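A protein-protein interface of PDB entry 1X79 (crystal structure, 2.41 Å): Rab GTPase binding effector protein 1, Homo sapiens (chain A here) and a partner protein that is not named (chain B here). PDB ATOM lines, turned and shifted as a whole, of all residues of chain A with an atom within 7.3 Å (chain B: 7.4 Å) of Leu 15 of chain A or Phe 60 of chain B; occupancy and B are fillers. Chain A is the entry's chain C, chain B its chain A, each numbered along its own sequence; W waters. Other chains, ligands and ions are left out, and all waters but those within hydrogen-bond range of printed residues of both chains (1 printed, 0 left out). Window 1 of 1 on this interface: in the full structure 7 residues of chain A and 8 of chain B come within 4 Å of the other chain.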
ATOM      1  N   LYS A   9      31.849 -13.095   7.005  1.00  0.00           N
ATOM      2  CA  LYS A   9      31.200 -14.312   7.457  1.00  0.00           C
ATOM      3  C   LYS A   9      29.727 -14.006   7.771  1.00  0.00           C
ATOM      4  O   LYS A   9      28.812 -14.762   7.409  1.00  0.00           O
ATOM      5  CB  LYS A   9      31.907 -14.856   8.698  1.00  0.00           C
ATOM      6  CG  LYS A   9      31.619 -16.344   8.970  1.00  0.00           C
ATOM      7  CD  LYS A   9      32.267 -16.881  10.279  1.00  0.00           C
ATOM      8  CE  LYS A   9      31.431 -16.578  11.539  1.00  0.00           C
ATOM      9  NZ  LYS A   9      30.106 -17.295  11.601  1.00  0.00           N
ATOM     10  N   LYS A  10      29.508 -12.878   8.427  1.00  0.00           N
ATOM     11  CA  LYS A  10      28.198 -12.485   8.915  1.00  0.00           C
ATOM     12  C   LYS A  10      27.201 -12.227   7.777  1.00  0.00           C
ATOM     13  O   LYS A  10      26.049 -12.646   7.848  1.00  0.00           O
ATOM     14  CB  LYS A  10      28.366 -11.232   9.748  1.00  0.00           C
ATOM     15  CG  LYS A  10      27.255 -10.909  10.697  1.00  0.00           C
ATOM     16  CD  LYS A  10      27.750  -9.821  11.656  1.00  0.00           C
ATOM     17  CE  LYS A  10      29.056 -10.261  12.347  1.00  0.00           C
ATOM     18  NZ  LYS A  10      29.743  -9.176  13.112  1.00  0.00           N
ATOM     19  N   LEU A  11      27.644 -11.515   6.743  1.00  0.00           N
ATOM     20  CA  LEU A  11      26.863 -11.357   5.530  1.00  0.00           C
ATOM     21  C   LEU A  11      26.667 -12.688   4.799  1.00  0.00           C
ATOM     22  O   LEU A  11      25.602 -12.961   4.255  1.00  0.00           O
ATOM     23  CB  LEU A  11      27.535 -10.375   4.574  1.00  0.00           C
ATOM     24  CG  LEU A  11      27.520  -8.894   4.905  1.00  0.00           C
ATOM     25  CD1 LEU A  11      28.596  -8.215   4.098  1.00  0.00           C
ATOM     26  CD2 LEU A  11      26.186  -8.288   4.591  1.00  0.00           C
ATOM     27  N   GLN A  12      27.695 -13.513   4.747  1.00  0.00           N
ATOM     28  CA  GLN A  12      27.523 -14.781   4.073  1.00  0.00           C
ATOM     29  C   GLN A  12      26.376 -15.556   4.681  1.00  0.00           C
ATOM     30  O   GLN A  12      25.570 -16.088   3.945  1.00  0.00           O
ATOM     31  CB  GLN A  12      28.807 -15.592   4.125  1.00  0.00           C
ATOM     32  CG  GLN A  12      29.852 -15.060   3.157  1.00  0.00           C
ATOM     33  CD  GLN A  12      31.141 -15.823   3.223  1.00  0.00           C
ATOM     34  OE1 GLN A  12      31.799 -15.872   4.263  1.00  0.00           O
ATOM     35  NE2 GLN A  12      31.513 -16.431   2.109  1.00  0.00           N
ATOM     36  N   LEU A  13      26.277 -15.592   6.010  1.00  0.00           N
ATOM     37  CA  LEU A  13      25.196 -16.333   6.655  1.00  0.00           C
ATOM     38  C   LEU A  13      23.833 -15.711   6.403  1.00  0.00           C
ATOM     39  O   LEU A  13      22.831 -16.408   6.291  1.00  0.00           O
ATOM     40  CB  LEU A  13      25.422 -16.436   8.163  1.00  0.00           C
ATOM     41  CG  LEU A  13      26.684 -17.212   8.560  1.00  0.00           C
ATOM     42  CD1 LEU A  13      26.824 -17.241  10.069  1.00  0.00           C
ATOM     43  CD2 LEU A  13      26.619 -18.636   8.019  1.00  0.00           C
ATOM     44  N   MET A  14      23.791 -14.392   6.331  1.00  0.00           N
ATOM     45  CA  MET A  14      22.568 -13.707   5.967  1.00  0.00           C
ATOM     46  C   MET A  14      22.222 -14.074   4.524  1.00  0.00           C
ATOM     47  O   MET A  14      21.064 -14.323   4.210  1.00  0.00           O
ATOM     48  CB  MET A  14      22.759 -12.200   6.076  1.00  0.00           C
ATOM     49  CG  MET A  14      22.316 -11.560   7.377  1.00  0.00           C
ATOM     50  SD  MET A  14      22.544  -9.739   7.347  1.00  0.00           S
ATOM     51  CE  MET A  14      24.305  -9.725   7.476  1.00  0.00           C
ATOM     52  N   LEU A  15      23.225 -14.099   3.647  1.00  0.00           N
ATOM     53  CA  LEU A  15      22.979 -14.313   2.220  1.00  0.00           C
ATOM     54  C   LEU A  15      22.466 -15.738   1.999  1.00  0.00           C
ATOM     55  O   LEU A  15      21.639 -15.980   1.142  1.00  0.00           O
ATOM     56  CB  LEU A  15      24.271 -14.141   1.434  1.00  0.00           C
ATOM     57  CG  LEU A  15      24.304 -13.422   0.090  1.00  0.00           C
ATOM     58  CD1 LEU A  15      25.293 -14.165  -0.794  1.00  0.00           C
ATOM     59  CD2 LEU A  15      22.966 -13.366  -0.565  1.00  0.00           C
ATOM     60  N   ARG A  16      22.981 -16.683   2.774  1.00  0.00           N
ATOM     61  CA  ARG A  16      22.588 -18.059   2.636  1.00  0.00           C
ATOM     62  C   ARG A  16      21.154 -18.208   3.102  1.00  0.00           C
ATOM     63  O   ARG A  16      20.394 -18.946   2.488  1.00  0.00           O
ATOM     64  CB  ARG A  16      23.503 -18.964   3.462  1.00  0.00           C
ATOM     65  CG  ARG A  16      23.086 -20.426   3.515  1.00  0.00           C
ATOM     66  CD  ARG A  16      22.989 -21.057   2.117  1.00  0.00           C
ATOM     67  NE  ARG A  16      23.312 -22.484   2.137  1.00  0.00           N
ATOM     68  CZ  ARG A  16      22.667 -23.405   2.854  1.00  0.00           C
ATOM     69  NH1 ARG A  16      21.642 -23.066   3.630  1.00  0.00           N
ATOM     70  NH2 ARG A  16      23.051 -24.678   2.802  1.00  0.00           N
ATOM     71  N   GLN A  17      20.781 -17.523   4.182  1.00  0.00           N
ATOM     72  CA  GLN A  17      19.386 -17.510   4.593  1.00  0.00           C
ATOM     73  C   GLN A  17      18.525 -16.998   3.430  1.00  0.00           C
ATOM     74  O   GLN A  17      17.515 -17.613   3.085  1.00  0.00           O
ATOM     75  CB  GLN A  17      19.178 -16.596   5.786  1.00  0.00           C
ATOM     76  CG  GLN A  17      19.924 -16.978   7.011  1.00  0.00           C
ATOM     77  CD  GLN A  17      19.553 -18.351   7.448  1.00  0.00           C
ATOM     78  OE1 GLN A  17      18.363 -18.673   7.598  1.00  0.00           O
ATOM     79  NE2 GLN A  17      20.559 -19.193   7.652  1.00  0.00           N
ATOM     80  N   ALA A  18      18.922 -15.878   2.827  1.00  0.00           N
ATOM     81  CA  ALA A  18      18.138 -15.296   1.749  1.00  0.00           C
ATOM     82  C   ALA A  18      18.024 -16.311   0.641  1.00  0.00           C
ATOM     83  O   ALA A  18      16.925 -16.581   0.151  1.00  0.00           O
ATOM     84  CB  ALA A  18      18.787 -14.053   1.218  1.00  0.00           C
ATOM     85  N   ASN A  19      19.156 -16.885   0.250  1.00  0.00           N
ATOM     86  CA  ASN A  19      19.168 -17.798  -0.886  1.00  0.00           C
ATOM     87  C   ASN A  19      18.300 -19.040  -0.693  1.00  0.00           C
ATOM     88  O   ASN A  19      17.612 -19.432  -1.608  1.00  0.00           O
ATOM     89  CB  ASN A  19      20.587 -18.231  -1.240  1.00  0.00           C
ATOM     90  CG  ASN A  19      20.693 -18.687  -2.693  1.00  0.00           C
ATOM     91  OD1 ASN A  19      20.331 -17.945  -3.618  1.00  0.00           O
ATOM     92  ND2 ASN A  19      21.174 -19.915  -2.905  1.00  0.00           N
ATOM     93  N   ASP A  20      18.326 -19.650   0.482  1.00  0.00           N
ATOM     94  CA  ASP A  20      17.498 -20.808   0.731  1.00  0.00           C
ATOM     95  C   ASP A  20      16.068 -20.429   0.469  1.00  0.00           C
ATOM     96  O   ASP A  20      15.286 -21.230  -0.041  1.00  0.00           O
ATOM     97  CB  ASP A  20      17.620 -21.281   2.182  1.00  0.00           C
ATOM     98  CG  ASP A  20      18.995 -21.865   2.487  1.00  0.00           C
ATOM     99  OD1 ASP A  20      19.768 -22.104   1.514  1.00  0.00           O
ATOM    100  OD2 ASP A  20      19.297 -22.091   3.688  1.00  0.00           O
ATOM    101  N   GLN A  21      15.729 -19.197   0.830  1.00  0.00           N
ATOM    102  CA  GLN A  21      14.355 -18.731   0.814  1.00  0.00           C
ATOM    103  C   GLN A  21      13.991 -18.460  -0.634  1.00  0.00           C
ATOM    104  O   GLN A  21      12.981 -18.910  -1.125  1.00  0.00           O
ATOM    105  CB  GLN A  21      14.247 -17.453   1.649  1.00  0.00           C
ATOM    106  CG  GLN A  21      12.907 -17.244   2.229  1.00  0.00           C
ATOM    107  CD  GLN A  21      12.535 -18.379   3.180  1.00  0.00           C
ATOM    108  OE1 GLN A  21      11.389 -18.844   3.192  1.00  0.00           O
ATOM    109  NE2 GLN A  21      13.499 -18.823   3.985  1.00  0.00           N
ATOM    110  N   LEU A  22      14.848 -17.730  -1.318  1.00  0.00           N
ATOM    111  CA  LEU A  22      14.700 -17.515  -2.736  1.00  0.00           C
ATOM    112  C   LEU A  22      14.436 -18.822  -3.472  1.00  0.00           C
ATOM    113  O   LEU A  22      13.554 -18.893  -4.309  1.00  0.00           O
ATOM    114  CB  LEU A  22      15.962 -16.890  -3.298  1.00  0.00           C
ATOM    115  CG  LEU A  22      15.770 -15.675  -4.180  1.00  0.00           C
ATOM    116  CD1 LEU A  22      17.018 -15.494  -5.010  1.00  0.00           C
ATOM    117  CD2 LEU A  22      14.585 -15.861  -5.093  1.00  0.00           C
ATOM    118  N   GLU A  23      15.199 -19.857  -3.161  1.00  0.00           N
ATOM    119  CA  GLU A  23      15.162 -21.064  -3.967  1.00  0.00           C
ATOM    120  C   GLU A  23      13.861 -21.774  -3.779  1.00  0.00           C
ATOM    121  O   GLU A  23      13.242 -22.209  -4.741  1.00  0.00           O
ATOM    122  CB  GLU A  23      16.306 -21.988  -3.602  1.00  0.00           C
ATOM    123  CG  GLU A  23      17.633 -21.302  -3.820  1.00  0.00           C
ATOM    124  CD  GLU A  23      18.791 -22.245  -3.947  1.00  0.00           C
ATOM    125  OE1 GLU A  23      18.915 -23.165  -3.080  1.00  0.00           O
ATOM    126  OE2 GLU A  23      19.570 -22.039  -4.924  1.00  0.00           O
ATOM    127  N   GLU B  53      19.042 -14.453 -15.482  1.00  0.00           N
ATOM    128  CA  GLU B  53      18.424 -14.072 -14.234  1.00  0.00           C
ATOM    129  C   GLU B  53      18.408 -15.186 -13.209  1.00  0.00           C
ATOM    130  O   GLU B  53      18.475 -14.933 -12.013  1.00  0.00           O
ATOM    131  CB  GLU B  53      17.001 -13.608 -14.470  1.00  0.00           C
ATOM    132  CG  GLU B  53      16.860 -12.117 -14.520  1.00  0.00           C
ATOM    133  CD  GLU B  53      15.426 -11.705 -14.411  1.00  0.00           C
ATOM    134  OE1 GLU B  53      14.679 -11.948 -15.384  1.00  0.00           O
ATOM    135  OE2 GLU B  53      15.044 -11.158 -13.347  1.00  0.00           O
ATOM    136  N   MET B  55      20.512 -17.496 -12.899  1.00  0.00           N
ATOM    137  CA  MET B  55      21.858 -17.731 -12.431  1.00  0.00           C
ATOM    138  C   MET B  55      22.213 -17.006 -11.136  1.00  0.00           C
ATOM    139  O   MET B  55      23.133 -17.427 -10.437  1.00  0.00           O
ATOM    140  CB  MET B  55      22.864 -17.347 -13.502  1.00  0.00           C
ATOM    141  CG  MET B  55      23.106 -18.428 -14.529  1.00  0.00           C
ATOM    142  SD  MET B  55      23.762 -19.918 -13.766  1.00  0.00           S
ATOM    143  CE  MET B  55      25.428 -19.385 -13.359  1.00  0.00           C
ATOM    144  N   ARG B  56      21.514 -15.929 -10.793  1.00  0.00           N
ATOM    145  CA  ARG B  56      21.874 -15.214  -9.580  1.00  0.00           C
ATOM    146  C   ARG B  56      21.783 -16.080  -8.313  1.00  0.00           C
ATOM    147  O   ARG B  56      22.696 -16.087  -7.466  1.00  0.00           O
ATOM    148  CB  ARG B  56      21.007 -13.992  -9.418  1.00  0.00           C
ATOM    149  CG  ARG B  56      20.909 -13.179 -10.658  1.00  0.00           C
ATOM    150  CD  ARG B  56      20.582 -11.751 -10.314  1.00  0.00           C
ATOM    151  NE  ARG B  56      21.820 -10.998 -10.175  1.00  0.00           N
ATOM    152  CZ  ARG B  56      21.899  -9.677 -10.276  1.00  0.00           C
ATOM    153  NH1 ARG B  56      20.804  -8.954 -10.505  1.00  0.00           N
ATOM    154  NH2 ARG B  56      23.081  -9.086 -10.201  1.00  0.00           N
ATOM    155  N   PRO B  57      20.682 -16.821  -8.157  1.00  0.00           N
ATOM    156  CA  PRO B  57      20.590 -17.645  -6.953  1.00  0.00           C
ATOM    157  C   PRO B  57      21.852 -18.476  -6.837  1.00  0.00           C
ATOM    158  O   PRO B  57      22.377 -18.710  -5.736  1.00  0.00           O
ATOM    159  CB  PRO B  57      19.356 -18.494  -7.222  1.00  0.00           C
ATOM    160  CG  PRO B  57      18.493 -17.598  -8.004  1.00  0.00           C
ATOM    161  CD  PRO B  57      19.459 -16.933  -8.967  1.00  0.00           C
ATOM    162  N   THR B  58      22.340 -18.910  -7.995  1.00  0.00           N
ATOM    163  CA  THR B  58      23.463 -19.843  -8.048  1.00  0.00           C
ATOM    164  C   THR B  58      24.696 -19.132  -7.518  1.00  0.00           C
ATOM    165  O   THR B  58      25.365 -19.633  -6.615  1.00  0.00           O
ATOM    166  CB  THR B  58      23.704 -20.319  -9.480  1.00  0.00           C
ATOM    167  OG1 THR B  58      22.496 -20.905  -9.996  1.00  0.00           O
ATOM    168  CG2 THR B  58      24.857 -21.323  -9.527  1.00  0.00           C
ATOM    169  N   LEU B  59      24.955 -17.938  -8.050  1.00  0.00           N
ATOM    170  CA  LEU B  59      26.002 -17.068  -7.518  1.00  0.00           C
ATOM    171  C   LEU B  59      25.811 -16.742  -6.051  1.00  0.00           C
ATOM    172  O   LEU B  59      26.794 -16.730  -5.317  1.00  0.00           O
ATOM    173  CB  LEU B  59      26.107 -15.755  -8.307  1.00  0.00           C
ATOM    174  CG  LEU B  59      26.845 -15.724  -9.660  1.00  0.00           C
ATOM    175  CD1 LEU B  59      27.566 -17.032  -9.966  1.00  0.00           C
ATOM    176  CD2 LEU B  59      25.866 -15.489 -10.705  1.00  0.00           C
ATOM    177  N   PHE B  60      24.575 -16.473  -5.612  1.00  0.00           N
ATOM    178  CA  PHE B  60      24.352 -16.126  -4.198  1.00  0.00           C
ATOM    179  C   PHE B  60      24.805 -17.287  -3.328  1.00  0.00           C
ATOM    180  O   PHE B  60      25.524 -17.106  -2.344  1.00  0.00           O
ATOM    181  CB  PHE B  60      22.861 -15.881  -3.871  1.00  0.00           C
ATOM    182  CG  PHE B  60      22.281 -14.674  -4.521  1.00  0.00           C
ATOM    183  CD1 PHE B  60      23.113 -13.625  -4.956  1.00  0.00           C
ATOM    184  CD2 PHE B  60      20.908 -14.597  -4.747  1.00  0.00           C
ATOM    185  CE1 PHE B  60      22.583 -12.539  -5.611  1.00  0.00           C
ATOM    186  CE2 PHE B  60      20.357 -13.505  -5.408  1.00  0.00           C
ATOM    187  CZ  PHE B  60      21.188 -12.470  -5.848  1.00  0.00           C
ATOM    188  N   ARG B  61      24.347 -18.482  -3.687  1.00  0.00           N
ATOM    189  CA  ARG B  61      24.629 -19.630  -2.870  1.00  0.00           C
ATOM    190  C   ARG B  61      26.131 -19.868  -2.830  1.00  0.00           C
ATOM    191  O   ARG B  61      26.689 -20.104  -1.765  1.00  0.00           O
ATOM    192  CB  ARG B  61      23.930 -20.862  -3.414  1.00  0.00           C
ATOM    193  CG  ARG B  61      24.272 -22.073  -2.618  1.00  0.00           C
ATOM    194  CD  ARG B  61      24.041 -21.817  -1.124  1.00  0.00           C
ATOM    195  NE  ARG B  61      24.625 -22.884  -0.313  1.00  0.00           N
ATOM    196  CZ  ARG B  61      24.149 -24.131  -0.237  1.00  0.00           C
ATOM    197  NH1 ARG B  61      23.063 -24.491  -0.916  1.00  0.00           N
ATOM    198  NH2 ARG B  61      24.780 -25.033   0.506  1.00  0.00           N
ATOM    199  N   LEU B  62      26.791 -19.805  -3.986  1.00  0.00           N
ATOM    200  CA  LEU B  62      28.239 -20.015  -4.033  1.00  0.00           C
ATOM    201  C   LEU B  62      28.924 -19.023  -3.103  1.00  0.00           C
ATOM    202  O   LEU B  62      29.660 -19.414  -2.192  1.00  0.00           O
ATOM    203  CB  LEU B  62      28.771 -19.851  -5.469  1.00  0.00           C
ATOM    204  CG  LEU B  62      28.391 -20.961  -6.479  1.00  0.00           C
ATOM    205  CD1 LEU B  62      28.793 -20.563  -7.883  1.00  0.00           C
ATOM    206  CD2 LEU B  62      29.056 -22.280  -6.108  1.00  0.00           C
ATOM    207  N   ALA B  63      28.648 -17.740  -3.311  1.00  0.00           N
ATOM    208  CA  ALA B  63      29.290 -16.711  -2.527  1.00  0.00           C
ATOM    209  C   ALA B  63      29.066 -16.949  -1.044  1.00  0.00           C
ATOM    210  O   ALA B  63      29.959 -16.712  -0.233  1.00  0.00           O
ATOM    211  CB  ALA B  63      28.776 -15.372  -2.927  1.00  0.00           C
ATOM    212  N   SER B  64      27.888 -17.422  -0.666  1.00  0.00           N
ATOM    213  CA  SER B  64      27.650 -17.612   0.751  1.00  0.00           C
ATOM    214  C   SER B  64      28.457 -18.786   1.291  1.00  0.00           C
ATOM    215  O   SER B  64      28.455 -19.043   2.488  1.00  0.00           O
ATOM    216  CB  SER B  64      26.174 -17.843   1.018  1.00  0.00           C
ATOM    217  OG  SER B  64      25.726 -18.981   0.329  1.00  0.00           O
ATOM    218  N   ASP B  65      29.157 -19.493   0.411  1.00  0.00           N
ATOM    219  CA  ASP B  65      29.784 -20.757   0.791  1.00  0.00           C
ATOM    220  C   ASP B  65      31.300 -20.739   0.796  1.00  0.00           C
ATOM    221  O   ASP B  65      31.928 -21.736   1.133  1.00  0.00           O
ATOM    222  CB  ASP B  65      29.322 -21.883  -0.133  1.00  0.00           C
ATOM    223  CG  ASP B  65      28.282 -22.757   0.507  1.00  0.00           C
ATOM    224  OD1 ASP B  65      28.409 -22.977   1.727  1.00  0.00           O
ATOM    225  OD2 ASP B  65      27.361 -23.229  -0.200  1.00  0.00           O
ATOM    226  N   THR B  66      31.872 -19.606   0.402  1.00  0.00           N
ATOM    227  CA  THR B  66      33.313 -19.437   0.343  1.00  0.00           C
ATOM    228  C   THR B  66      33.887 -19.234   1.726  1.00  0.00           C
ATOM    229  O   THR B  66      34.074 -18.105   2.177  1.00  0.00           O
ATOM    230  CB  THR B  66      33.695 -18.225  -0.490  1.00  0.00           C
ATOM    231  OG1 THR B  66      33.356 -18.463  -1.857  1.00  0.00           O
ATOM    232  CG2 THR B  66      35.188 -17.964  -0.376  1.00  0.00           C
ATOM    233  N   ILE B  76      33.725 -15.204  -7.677  1.00  0.00           N
ATOM    234  CA  ILE B  76      32.260 -15.238  -7.674  1.00  0.00           C
ATOM    235  C   ILE B  76      31.742 -13.829  -7.858  1.00  0.00           C
ATOM    236  O   ILE B  76      31.002 -13.546  -8.817  1.00  0.00           O
ATOM    237  CB  ILE B  76      31.655 -15.713  -6.348  1.00  0.00           C
ATOM    238  CG1 ILE B  76      32.365 -16.962  -5.807  1.00  0.00           C
ATOM    239  CG2 ILE B  76      30.173 -15.959  -6.569  1.00  0.00           C
ATOM    240  CD1 ILE B  76      31.994 -18.214  -6.486  1.00  0.00           C
ATOM    241  N   LEU B  77      32.132 -12.951  -6.932  1.00  0.00           N
ATOM    242  CA  LEU B  77      31.612 -11.587  -6.916  1.00  0.00           C
ATOM    243  C   LEU B  77      31.940 -10.853  -8.215  1.00  0.00           C
ATOM    244  O   LEU B  77      31.154 -10.029  -8.681  1.00  0.00           O
ATOM    245  CB  LEU B  77      32.151 -10.826  -5.706  1.00  0.00           C
ATOM    246  CG  LEU B  77      31.859 -11.545  -4.380  1.00  0.00           C
ATOM    247  CD1 LEU B  77      32.668 -10.963  -3.243  1.00  0.00           C
ATOM    248  CD2 LEU B  77      30.401 -11.431  -4.065  1.00  0.00           C
ATOM    249  N   ASN B  80      29.354 -11.938 -10.503  1.00  0.00           N
ATOM    250  CA  ASN B  80      28.101 -11.279 -10.179  1.00  0.00           C
ATOM    251  C   ASN B  80      28.092  -9.852 -10.735  1.00  0.00           C
ATOM    252  O   ASN B  80      27.072  -9.405 -11.297  1.00  0.00           O
ATOM    253  CB  ASN B  80      27.861 -11.233  -8.672  1.00  0.00           C
ATOM    254  CG  ASN B  80      26.449 -10.796  -8.332  1.00  0.00           C
ATOM    255  OD1 ASN B  80      25.494 -11.390  -8.811  1.00  0.00           O
ATOM    256  ND2 ASN B  80      26.308  -9.760  -7.512  1.00  0.00           N
HETATM  257  O   HOH W   1      25.913 -21.402   1.758  1.00  0.00           O
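Of the 16 printed residues of chain B, 6 touch a printed residue of chain A.
Of the 15 printed residues of chain A, 5 touch a printed residue of chain B.
Hydrophobic or aromatic side chains of chain A that line the printed part of chain B: Leu 15 and Leu 22.
Along chain A the printed residues that touch a printed residue of chain B span positions 12 to 22.
Among the printed residues, 11 pairs touch across the chains.
Of the printed residues of chain B, Gln 12 of chain A touches Ala 63, Ser 64 and Thr 66.
Leu 15 of chain A touches just one residue of chain B: Phe 60 (3.3 Å).
Thr 58 of chain B touches none of the printed residues of chain A.
Of chain A, only Leu 15 (3.3 Å), Asn 19 (3.3 Å) and Leu 22 (3.9 Å) come within 4 Å of Phe 60 of chain B.
Printed residues of chain A within 4 Å of Arg 61 of chain B: Arg 16 (2.8 Å) and Asn 19 (3.0 Å).
Leu 62 of chain B touches none of the printed residues of chain A.
Printed residues of chain A within 4 Å of Ala 63 of chain B: Gln 12 (2.8 Å).
Of the printed residues of chain A, Thr 66 of chain B touches Gln 12 (3.1 Å).
The nearest residue of chain B that does not touch Leu 15 of chain A is Ser 64 of chain B (4.2 Å).
The nearest residue of chain A that does not touch Phe 60 of chain B is Arg 16 of chain A (5.7 Å).
The nearest printed residue of chain A that does not touch Arg 61 of chain B is Asp 20 of chain A (4.7 Å).
Water W1 lies within hydrogen-bond range of the side-chain hydroxyl of Ser 64 of chain B, the guanidinium group of Arg 16 of chain A, the guanidinium group of Arg 61 of chain B and the side-chain carboxylate of Asp 65 of chain B.
O of Pro 57 of chain B lies close to OD1 of Asn 19 of chain A, 3.0 Å away.
NE2 of Gln 12 of chain A sits at hydrogen-bond distance from O of Thr 66 of chain B (3.1 Å).
The side-chain amide nitrogen (NE2) of Gln 12 of chain A lies within hydrogen-bond range of the backbone carbonyl oxygen (O) of Ala 63 of chain B (2.8 Å).
NE of Arg 61 of chain B lies close to NE of Arg 16 of chain A, at 2.8 Å.
Gln 12 of chain A touches Ser 64 of chain B.
O of Phe 60 of chain B touches CD1 of Leu 15 of chain A, at 3.3 Å.
Ser 64 of chain B touches Arg 16 of chain A.
Asn 19 of chain A touches Phe 60 of chain B.
Arg 61 of chain B touches Asn 19 of chain A (CB to ND2, 3.0 Å).
Leu 22 of chain A touches Pro 57 of chain B.
CD1 of Leu 22 of chain A touches CE2 of Phe 60 of chain B (3.9 Å).
ND2 of Asn 19 of chain A sits at hydrogen-bond distance from OE2 of Glu 23 of chain A, at 3.3 Å.
The backbone carbonyl oxygen (O) of Phe 60 of chain B lies within hydrogen-bond range of the side-chain hydroxyl (OG) of Ser 64 of chain B.
O of Arg 61 of chain B sits at hydrogen-bond distance from OG of Ser 64 of chain B, at 2.6 Å.
NE of Arg 61 of chain B is in salt-bridge range of OD2 of Asp 65 of chain B (2.8 Å).
NH1 of Arg 16 of chain A is in salt-bridge range of OD2 of Asp 20 of chain A, at 2.5 Å.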
